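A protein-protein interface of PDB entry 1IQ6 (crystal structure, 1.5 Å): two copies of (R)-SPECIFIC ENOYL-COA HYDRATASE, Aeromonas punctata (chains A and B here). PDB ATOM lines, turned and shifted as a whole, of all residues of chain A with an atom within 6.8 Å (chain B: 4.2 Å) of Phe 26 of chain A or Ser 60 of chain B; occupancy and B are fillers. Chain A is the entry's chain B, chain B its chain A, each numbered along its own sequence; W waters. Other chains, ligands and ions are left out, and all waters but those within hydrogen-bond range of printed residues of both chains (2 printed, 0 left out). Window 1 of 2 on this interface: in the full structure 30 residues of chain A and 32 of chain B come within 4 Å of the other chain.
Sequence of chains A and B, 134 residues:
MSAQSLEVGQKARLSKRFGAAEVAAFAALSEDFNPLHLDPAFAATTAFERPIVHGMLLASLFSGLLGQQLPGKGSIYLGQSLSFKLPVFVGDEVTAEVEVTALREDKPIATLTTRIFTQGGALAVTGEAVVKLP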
ATOM      1  N   ALA A  21     -18.725   5.869   6.602  1.00  0.00           N
ATOM      2  CA  ALA A  21     -19.528   4.708   6.247  1.00  0.00           C
ATOM      3  C   ALA A  21     -18.698   3.628   5.565  1.00  0.00           C
ATOM      4  O   ALA A  21     -18.852   2.440   5.850  1.00  0.00           O
ATOM      5  CB  ALA A  21     -20.690   5.126   5.345  1.00  0.00           C
ATOM      6  N   GLU A  22     -17.817   4.040   4.661  1.00  0.00           N
ATOM      7  CA  GLU A  22     -16.986   3.076   3.951  1.00  0.00           C
ATOM      8  C   GLU A  22     -15.978   2.424   4.891  1.00  0.00           C
ATOM      9  O   GLU A  22     -15.766   1.211   4.842  1.00  0.00           O
ATOM     10  CB  GLU A  22     -16.266   3.755   2.781  1.00  0.00           C
ATOM     11  CG  GLU A  22     -17.203   4.158   1.648  1.00  0.00           C
ATOM     12  CD  GLU A  22     -18.020   5.395   1.966  1.00  0.00           C
ATOM     13  OE1 GLU A  22     -19.166   5.496   1.477  1.00  0.00           O
ATOM     14  OE2 GLU A  22     -17.511   6.275   2.692  1.00  0.00           O
ATOM     15  N   VAL A  23     -15.361   3.227   5.749  1.00  0.00           N
ATOM     16  CA  VAL A  23     -14.394   2.695   6.699  1.00  0.00           C
ATOM     17  C   VAL A  23     -15.085   1.719   7.654  1.00  0.00           C
ATOM     18  O   VAL A  23     -14.521   0.682   8.006  1.00  0.00           O
ATOM     19  CB  VAL A  23     -13.712   3.834   7.485  1.00  0.00           C
ATOM     20  CG1 VAL A  23     -12.805   3.256   8.567  1.00  0.00           C
ATOM     21  CG2 VAL A  23     -12.897   4.701   6.526  1.00  0.00           C
ATOM     22  N   ALA A  24     -16.311   2.042   8.057  1.00  0.00           N
ATOM     23  CA  ALA A  24     -17.059   1.160   8.948  1.00  0.00           C
ATOM     24  C   ALA A  24     -17.371  -0.164   8.251  1.00  0.00           C
ATOM     25  O   ALA A  24     -17.277  -1.233   8.859  1.00  0.00           O
ATOM     26  CB  ALA A  24     -18.353   1.837   9.392  1.00  0.00           C
ATOM     27  N   ALA A  25     -17.744  -0.097   6.975  1.00  0.00           N
ATOM     28  CA  ALA A  25     -18.053  -1.301   6.217  1.00  0.00           C
ATOM     29  C   ALA A  25     -16.800  -2.164   6.066  1.00  0.00           C
ATOM     30  O   ALA A  25     -16.869  -3.391   6.136  1.00  0.00           O
ATOM     31  CB  ALA A  25     -18.607  -0.931   4.842  1.00  0.00           C
ATOM     32  N   PHE A  26     -15.651  -1.525   5.866  1.00  0.00           N
ATOM     33  CA  PHE A  26     -14.417  -2.286   5.719  1.00  0.00           C
ATOM     34  C   PHE A  26     -14.030  -2.920   7.048  1.00  0.00           C
ATOM     35  O   PHE A  26     -13.532  -4.042   7.082  1.00  0.00           O
ATOM     36  CB  PHE A  26     -13.261  -1.409   5.233  1.00  0.00           C
ATOM     37  CG  PHE A  26     -12.003  -2.190   4.965  1.00  0.00           C
ATOM     38  CD1 PHE A  26     -11.898  -2.992   3.833  1.00  0.00           C
ATOM     39  CD2 PHE A  26     -10.942  -2.163   5.869  1.00  0.00           C
ATOM     40  CE1 PHE A  26     -10.755  -3.759   3.605  1.00  0.00           C
ATOM     41  CE2 PHE A  26      -9.797  -2.924   5.652  1.00  0.00           C
ATOM     42  CZ  PHE A  26      -9.705  -3.724   4.517  1.00  0.00           C
ATOM     43  N   ALA A  27     -14.255  -2.195   8.139  1.00  0.00           N
ATOM     44  CA  ALA A  27     -13.943  -2.714   9.464  1.00  0.00           C
ATOM     45  C   ALA A  27     -14.747  -3.996   9.694  1.00  0.00           C
ATOM     46  O   ALA A  27     -14.211  -4.995  10.168  1.00  0.00           O
ATOM     47  CB  ALA A  27     -14.284  -1.677  10.528  1.00  0.00           C
ATOM     48  N   ALA A  28     -16.031  -3.964   9.339  1.00  0.00           N
ATOM     49  CA  ALA A  28     -16.895  -5.130   9.503  1.00  0.00           C
ATOM     50  C   ALA A  28     -16.454  -6.329   8.656  1.00  0.00           C
ATOM     51  O   ALA A  28     -16.490  -7.466   9.120  1.00  0.00           O
ATOM     52  CB  ALA A  28     -18.337  -4.757   9.168  1.00  0.00           C
ATOM     53  N   LEU A  29     -16.045  -6.082   7.413  1.00  0.00           N
ATOM     54  CA  LEU A  29     -15.608  -7.156   6.526  1.00  0.00           C
ATOM     55  C   LEU A  29     -14.264  -7.752   6.933  1.00  0.00           C
ATOM     56  O   LEU A  29     -14.082  -8.972   6.916  1.00  0.00           O
ATOM     57  CB  LEU A  29     -15.499  -6.644   5.086  1.00  0.00           C
ATOM     58  CG  LEU A  29     -16.794  -6.306   4.344  1.00  0.00           C
ATOM     59  CD1 LEU A  29     -16.468  -5.489   3.106  1.00  0.00           C
ATOM     60  CD2 LEU A  29     -17.517  -7.593   3.971  1.00  0.00           C
ATOM     61  N   SER A  30     -13.331  -6.880   7.304  1.00  0.00           N
ATOM     62  CA  SER A  30     -11.979  -7.284   7.682  1.00  0.00           C
ATOM     63  C   SER A  30     -11.831  -7.717   9.133  1.00  0.00           C
ATOM     64  O   SER A  30     -10.862  -8.386   9.486  1.00  0.00           O
ATOM     65  CB  SER A  30     -11.016  -6.119   7.438  1.00  0.00           C
ATOM     66  OG  SER A  30     -11.304  -5.050   8.328  1.00  0.00           O
ATOM     67  N   GLU A  31     -12.793  -7.324   9.961  1.00  0.00           N
ATOM     68  CA  GLU A  31     -12.778  -7.604  11.395  1.00  0.00           C
ATOM     69  C   GLU A  31     -11.753  -6.697  12.086  1.00  0.00           C
ATOM     70  O   GLU A  31     -11.405  -6.915  13.247  1.00  0.00           O
ATOM     71  CB  GLU A  31     -12.447  -9.078  11.674  1.00  0.00           C
ATOM     72  CG  GLU A  31     -13.459 -10.064  11.100  1.00  0.00           C
ATOM     73  CD  GLU A  31     -14.838  -9.925  11.722  1.00  0.00           C
ATOM     74  OE1 GLU A  31     -15.813 -10.391  11.096  1.00  0.00           O
ATOM     75  OE2 GLU A  31     -14.946  -9.363  12.836  1.00  0.00           O
ATOM     76  N   ASP A  32     -11.276  -5.676  11.372  1.00  0.00           N
ATOM     77  CA  ASP A  32     -10.299  -4.739  11.931  1.00  0.00           C
ATOM     78  C   ASP A  32     -10.971  -3.484  12.474  1.00  0.00           C
ATOM     79  O   ASP A  32     -11.201  -2.517  11.739  1.00  0.00           O
ATOM     80  CB  ASP A  32      -9.254  -4.331  10.883  1.00  0.00           C
ATOM     81  CG  ASP A  32      -8.183  -3.406  11.458  1.00  0.00           C
ATOM     82  OD1 ASP A  32      -8.254  -3.084  12.661  1.00  0.00           O
ATOM     83  OD2 ASP A  32      -7.263  -3.009  10.710  1.00  0.00           O
ATOM     84  N   PHE A  33     -11.281  -3.504  13.764  1.00  0.00           N
ATOM     85  CA  PHE A  33     -11.918  -2.371  14.414  1.00  0.00           C
ATOM     86  C   PHE A  33     -10.905  -1.555  15.223  1.00  0.00           C
ATOM     87  O   PHE A  33     -11.238  -0.980  16.259  1.00  0.00           O
ATOM     88  CB  PHE A  33     -13.053  -2.856  15.320  1.00  0.00           C
ATOM     89  CG  PHE A  33     -14.102  -3.652  14.598  1.00  0.00           C
ATOM     90  CD1 PHE A  33     -13.962  -5.028  14.433  1.00  0.00           C
ATOM     91  CD2 PHE A  33     -15.218  -3.023  14.058  1.00  0.00           C
ATOM     92  CE1 PHE A  33     -14.923  -5.767  13.736  1.00  0.00           C
ATOM     93  CE2 PHE A  33     -16.184  -3.749  13.359  1.00  0.00           C
ATOM     94  CZ  PHE A  33     -16.035  -5.123  13.199  1.00  0.00           C
ATOM     95  N   HIS A  54      -8.116   2.558   6.717  1.00  0.00           N
ATOM     96  CA  HIS A  54      -7.308   1.334   6.746  1.00  0.00           C
ATOM     97  C   HIS A  54      -6.426   1.272   5.508  1.00  0.00           C
ATOM     98  O   HIS A  54      -6.908   1.449   4.393  1.00  0.00           O
ATOM     99  CB  HIS A  54      -8.176   0.079   6.699  1.00  0.00           C
ATOM    100  CG  HIS A  54      -9.125  -0.067   7.842  1.00  0.00           C
ATOM    101  ND1 HIS A  54     -10.212   0.761   8.020  1.00  0.00           N
ATOM    102  CD2 HIS A  54      -9.196  -1.000   8.820  1.00  0.00           C
ATOM    103  CE1 HIS A  54     -10.916   0.340   9.056  1.00  0.00           C
ATOM    104  NE2 HIS A  54     -10.320  -0.727   9.558  1.00  0.00           N
ATOM    105  N   GLY A  55      -5.144   0.985   5.703  1.00  0.00           N
ATOM    106  CA  GLY A  55      -4.255   0.882   4.560  1.00  0.00           C
ATOM    107  C   GLY A  55      -4.736  -0.204   3.609  1.00  0.00           C
ATOM    108  O   GLY A  55      -4.629  -0.070   2.388  1.00  0.00           O
ATOM    109  N   MET A  56      -5.280  -1.289   4.154  1.00  0.00           N
ATOM    110  CA  MET A  56      -5.753  -2.369   3.300  1.00  0.00           C
ATOM    111  C   MET A  56      -7.030  -2.016   2.529  1.00  0.00           C
ATOM    112  O   MET A  56      -7.380  -2.687   1.557  1.00  0.00           O
ATOM    113  CB  MET A  56      -5.926  -3.660   4.107  1.00  0.00           C
ATOM    114  CG  MET A  56      -4.597  -4.344   4.469  1.00  0.00           C
ATOM    115  SD  MET A  56      -3.573  -4.864   3.042  1.00  0.00           S
ATOM    116  CE  MET A  56      -4.346  -6.440   2.676  1.00  0.00           C
ATOM    117  N   LEU A  57      -7.735  -0.973   2.966  1.00  0.00           N
ATOM    118  CA  LEU A  57      -8.918  -0.528   2.236  1.00  0.00           C
ATOM    119  C   LEU A  57      -8.384   0.295   1.053  1.00  0.00           C
ATOM    120  O   LEU A  57      -8.854   0.148  -0.076  1.00  0.00           O
ATOM    121  CB  LEU A  57      -9.837   0.328   3.128  1.00  0.00           C
ATOM    122  CG  LEU A  57     -11.045   0.984   2.434  1.00  0.00           C
ATOM    123  CD1 LEU A  57     -11.821  -0.044   1.626  1.00  0.00           C
ATOM    124  CD2 LEU A  57     -11.944   1.633   3.487  1.00  0.00           C
ATOM    125  N   LEU A  58      -7.392   1.145   1.318  1.00  0.00           N
ATOM    126  CA  LEU A  58      -6.790   1.945   0.252  1.00  0.00           C
ATOM    127  C   LEU A  58      -6.245   1.008  -0.829  1.00  0.00           C
ATOM    128  O   LEU A  58      -6.485   1.205  -2.019  1.00  0.00           O
ATOM    129  CB  LEU A  58      -5.638   2.797   0.797  1.00  0.00           C
ATOM    130  CG  LEU A  58      -5.928   3.838   1.879  1.00  0.00           C
ATOM    131  CD1 LEU A  58      -4.629   4.491   2.349  1.00  0.00           C
ATOM    132  CD2 LEU A  58      -6.880   4.877   1.321  1.00  0.00           C
ATOM    133  N   SER A  60      -7.155  -1.897  -1.633  1.00  0.00           N
ATOM    134  CA  SER A  60      -8.194  -2.625  -2.352  1.00  0.00           C
ATOM    135  C   SER A  60      -8.587  -1.954  -3.669  1.00  0.00           C
ATOM    136  O   SER A  60      -9.124  -2.607  -4.565  1.00  0.00           O
ATOM    137  CB  SER A  60      -9.423  -2.803  -1.458  1.00  0.00           C
ATOM    138  OG  SER A  60      -9.116  -3.647  -0.357  1.00  0.00           O
ATOM    139  N   LEU B  29     -16.700  -1.226  -2.324  1.00  0.00           N
ATOM    140  CA  LEU B  29     -15.597  -0.499  -1.708  1.00  0.00           C
ATOM    141  C   LEU B  29     -14.361  -0.431  -2.605  1.00  0.00           C
ATOM    142  O   LEU B  29     -13.758   0.631  -2.764  1.00  0.00           O
ATOM    143  CB  LEU B  29     -15.211  -1.157  -0.380  1.00  0.00           C
ATOM    144  CG  LEU B  29     -16.178  -1.005   0.793  1.00  0.00           C
ATOM    145  CD1 LEU B  29     -15.750  -1.932   1.926  1.00  0.00           C
ATOM    146  CD2 LEU B  29     -16.190   0.440   1.262  1.00  0.00           C
ATOM    147  N   MET B  56      -8.237  -9.731  -2.369  1.00  0.00           N
ATOM    148  CA  MET B  56      -8.028  -8.664  -1.396  1.00  0.00           C
ATOM    149  C   MET B  56      -9.040  -8.670  -0.258  1.00  0.00           C
ATOM    150  O   MET B  56      -8.799  -8.074   0.794  1.00  0.00           O
ATOM    151  CB  MET B  56      -8.004  -7.300  -2.089  1.00  0.00           C
ATOM    152  CG  MET B  56      -6.732  -7.051  -2.911  1.00  0.00           C
ATOM    153  SD  MET B  56      -5.202  -7.097  -1.934  1.00  0.00           S
ATOM    154  CE  MET B  56      -5.396  -5.597  -0.951  1.00  0.00           C
ATOM    155  N   LEU B  57     -10.178  -9.331  -0.458  1.00  0.00           N
ATOM    156  CA  LEU B  57     -11.156  -9.425   0.616  1.00  0.00           C
ATOM    157  C   LEU B  57     -10.589 -10.467   1.580  1.00  0.00           C
ATOM    158  O   LEU B  57     -10.662 -10.306   2.795  1.00  0.00           O
ATOM    159  CB  LEU B  57     -12.527  -9.864   0.094  1.00  0.00           C
ATOM    160  CG  LEU B  57     -13.584 -10.099   1.183  1.00  0.00           C
ATOM    161  CD1 LEU B  57     -13.642  -8.927   2.157  1.00  0.00           C
ATOM    162  CD2 LEU B  57     -14.933 -10.314   0.520  1.00  0.00           C
ATOM    163  N   LEU B  58     -10.004 -11.528   1.028  1.00  0.00           N
ATOM    164  CA  LEU B  58      -9.394 -12.559   1.857  1.00  0.00           C
ATOM    165  C   LEU B  58      -8.259 -11.919   2.656  1.00  0.00           C
ATOM    166  O   LEU B  58      -8.147 -12.113   3.865  1.00  0.00           O
ATOM    167  CB  LEU B  58      -8.833 -13.693   0.990  1.00  0.00           C
ATOM    168  CG  LEU B  58      -9.823 -14.535   0.175  1.00  0.00           C
ATOM    169  CD1 LEU B  58      -9.061 -15.545  -0.673  1.00  0.00           C
ATOM    170  CD2 LEU B  58     -10.789 -15.238   1.114  1.00  0.00           C
ATOM    171  N   ALA B  59      -7.425 -11.140   1.969  1.00  0.00           N
ATOM    172  CA  ALA B  59      -6.290 -10.478   2.606  1.00  0.00           C
ATOM    173  C   ALA B  59      -6.680  -9.469   3.685  1.00  0.00           C
ATOM    174  O   ALA B  59      -5.888  -9.190   4.588  1.00  0.00           O
ATOM    175  CB  ALA B  59      -5.430  -9.796   1.549  1.00  0.00           C
ATOM    176  N   SER B  60      -7.891  -8.924   3.595  1.00  0.00           N
ATOM    177  CA  SER B  60      -8.348  -7.944   4.580  1.00  0.00           C
ATOM    178  C   SER B  60      -8.358  -8.538   5.986  1.00  0.00           C
ATOM    179  O   SER B  60      -8.226  -7.810   6.975  1.00  0.00           O
ATOM    180  CB  SER B  60      -9.756  -7.433   4.229  1.00  0.00           C
ATOM    181  OG  SER B  60     -10.771  -8.357   4.598  1.00  0.00           O
ATOM    182  N   LEU B  61      -8.509  -9.860   6.072  1.00  0.00           N
ATOM    183  CA  LEU B  61      -8.535 -10.538   7.362  1.00  0.00           C
ATOM    184  C   LEU B  61      -7.229 -10.347   8.125  1.00  0.00           C
ATOM    185  O   LEU B  61      -7.212 -10.402   9.358  1.00  0.00           O
ATOM    186  CB  LEU B  61      -8.823 -12.029   7.168  1.00  0.00           C
ATOM    187  CG  LEU B  61     -10.220 -12.316   6.614  1.00  0.00           C
ATOM    188  CD1 LEU B  61     -10.407 -13.816   6.430  1.00  0.00           C
ATOM    189  CD2 LEU B  61     -11.264 -11.757   7.574  1.00  0.00           C
ATOM    190  N   PHE B  62      -6.137 -10.121   7.394  1.00  0.00           N
ATOM    191  CA  PHE B  62      -4.846  -9.887   8.032  1.00  0.00           C
ATOM    192  C   PHE B  62      -4.927  -8.570   8.814  1.00  0.00           C
ATOM    193  O   PHE B  62      -4.331  -8.428   9.880  1.00  0.00           O
ATOM    194  CB  PHE B  62      -3.730  -9.814   6.978  1.00  0.00           C
ATOM    195  CG  PHE B  62      -3.499 -11.111   6.232  1.00  0.00           C
ATOM    196  CD1 PHE B  62      -2.963 -11.096   4.947  1.00  0.00           C
ATOM    197  CD2 PHE B  62      -3.800 -12.341   6.815  1.00  0.00           C
ATOM    198  CE1 PHE B  62      -2.728 -12.283   4.247  1.00  0.00           C
ATOM    199  CE2 PHE B  62      -3.567 -13.534   6.123  1.00  0.00           C
ATOM    200  CZ  PHE B  62      -3.032 -13.508   4.840  1.00  0.00           C
ATOM    201  N   SER B  63      -5.676  -7.603   8.291  1.00  0.00           N
ATOM    202  CA  SER B  63      -5.817  -6.331   8.983  1.00  0.00           C
ATOM    203  C   SER B  63      -6.603  -6.583  10.277  1.00  0.00           C
ATOM    204  O   SER B  63      -6.310  -5.999  11.316  1.00  0.00           O
ATOM    205  CB  SER B  63      -6.540  -5.317   8.087  1.00  0.00           C
ATOM    206  OG  SER B  63      -6.294  -3.991   8.523  1.00  0.00           O
ATOM    207  N   GLY B  64      -7.594  -7.471  10.209  1.00  0.00           N
ATOM    208  CA  GLY B  64      -8.366  -7.788  11.398  1.00  0.00           C
ATOM    209  C   GLY B  64      -7.497  -8.440  12.465  1.00  0.00           C
ATOM    210  O   GLY B  64      -7.596  -8.119  13.650  1.00  0.00           O
HETATM  211  O   HOH W   1      -5.364  -1.902   7.034  1.00  0.00           O
HETATM  212  O   HOH W   2      -7.888  -5.827   2.171  1.00  0.00           O
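Hydrophobic or aromatic side chains of chain A that line the printed part of chain B: Phe 26, Leu 29 and Met 56.
Of the 10 printed residues of chain B, 7 touch a printed residue of chain A.
Among the printed residues, 12 pairs touch across the chains.
Phe 26 of chain A touches just these residues of chain B: Leu 29 and Ser 60.
Of chain A, only Phe 26 (3.7 Å) and Ser 30 (3.3 Å) come within 4 Å of Ser 60 of chain B.
Printed residues of chain A within 4 Å of Leu 29 of chain B: Glu 22 (3.6 Å), Phe 26 (3.96 Å) and Leu 29 (3.8 Å).
Printed residues of chain A within 4 Å of Ser 63 of chain B: Asp 32 (2.6 Å).
The nearest printed residue of chain B that does not touch Phe 26 of chain A is Ser 63 of chain B (4.7 Å).
The nearest residue of chain A that does not touch Ser 60 of chain B is Leu 29 of chain A (4.1 Å).
The nearest printed residue of chain A that does not touch Ser 63 of chain B is His 54 of chain A (4.2 Å).
The backbone carbonyl oxygen (O) of Asp 32 of chain A lies within hydrogen-bond range of a ring nitrogen (NE2) of His 54 of chain A.
The backbone carbonyl oxygen (O) of Ala 27 of chain A is in hydrogen-bond range of the side-chain hydroxyl (OG) of Ser 30 of chain A, at 3.4 Å.
OG of Ser 60 of chain B lies within hydrogen-bond range of O of Leu 57 of chain B, at 2.7 Å.
N of Asp 32 of chain A lies within hydrogen-bond range of O of Ala 27 of chain A (3.2 Å).
The side-chain hydroxyl of Ser 30 of chain A lies close to the backbone NH of Asp 32 of chain A (3.1 Å).
The backbone carbonyl oxygen of Met 56 of chain A lies within hydrogen-bond range of the side-chain hydroxyl of Ser 60 of chain A (2.8 Å).
Glu 22 of chain A touches Leu 29 of chain B (CB to CD2, 3.6 Å).
Phe 26 of chain A touches Leu 29 of chain B.
Phe 26 of chain A touches Ser 60 of chain B.
CD1 of Leu 29 of chain B touches CD1 of Leu 29 of chain A, 3.8 Å away.
Ser 60 of chain B touches Ser 30 of chain A (O to CB, 3.3 Å).
Leu 61 of chain B touches Ser 30 of chain A (CA to O, 3.8 Å).
Gly 64 of chain B touches Glu 31 of chain A (CA to C, 3.6 Å).
Asp 32 of chain A touches Gly 64 of chain B.
Met 56 of chain A touches Met 56 of chain B.
Met 56 of chain A touches Ala 59 of chain B.
Leu 29 of chain B touches its own counterpart, Leu 29 of chain A.
Met 56 of chain B touches its own counterpart, Met 56 of chain A.
Positions printed for both chains: 29, 56, 57, 58 and 60.
The backbone NH of Gly 64 of chain B sits close to the backbone carbonyl oxygen of Ser 30 of chain A, 3.5 Å away.
OG of Ser 63 of chain B is in hydrogen-bond range of OD2 of Asp 32 of chain A.
Water W1 lies within hydrogen-bond range of OG of Ser 63 of chain B, N of Met 56 of chain A and N of Gly 55 of chain A.
Water W2 lies within hydrogen-bond range of the backbone carbonyl oxygen of Met 56 of chain B (2.8 Å), the backbone carbonyl oxygen of Met 56 of chain A (3.2 Å) and the backbone NH of Ser 60 of chain B (3.4 Å).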
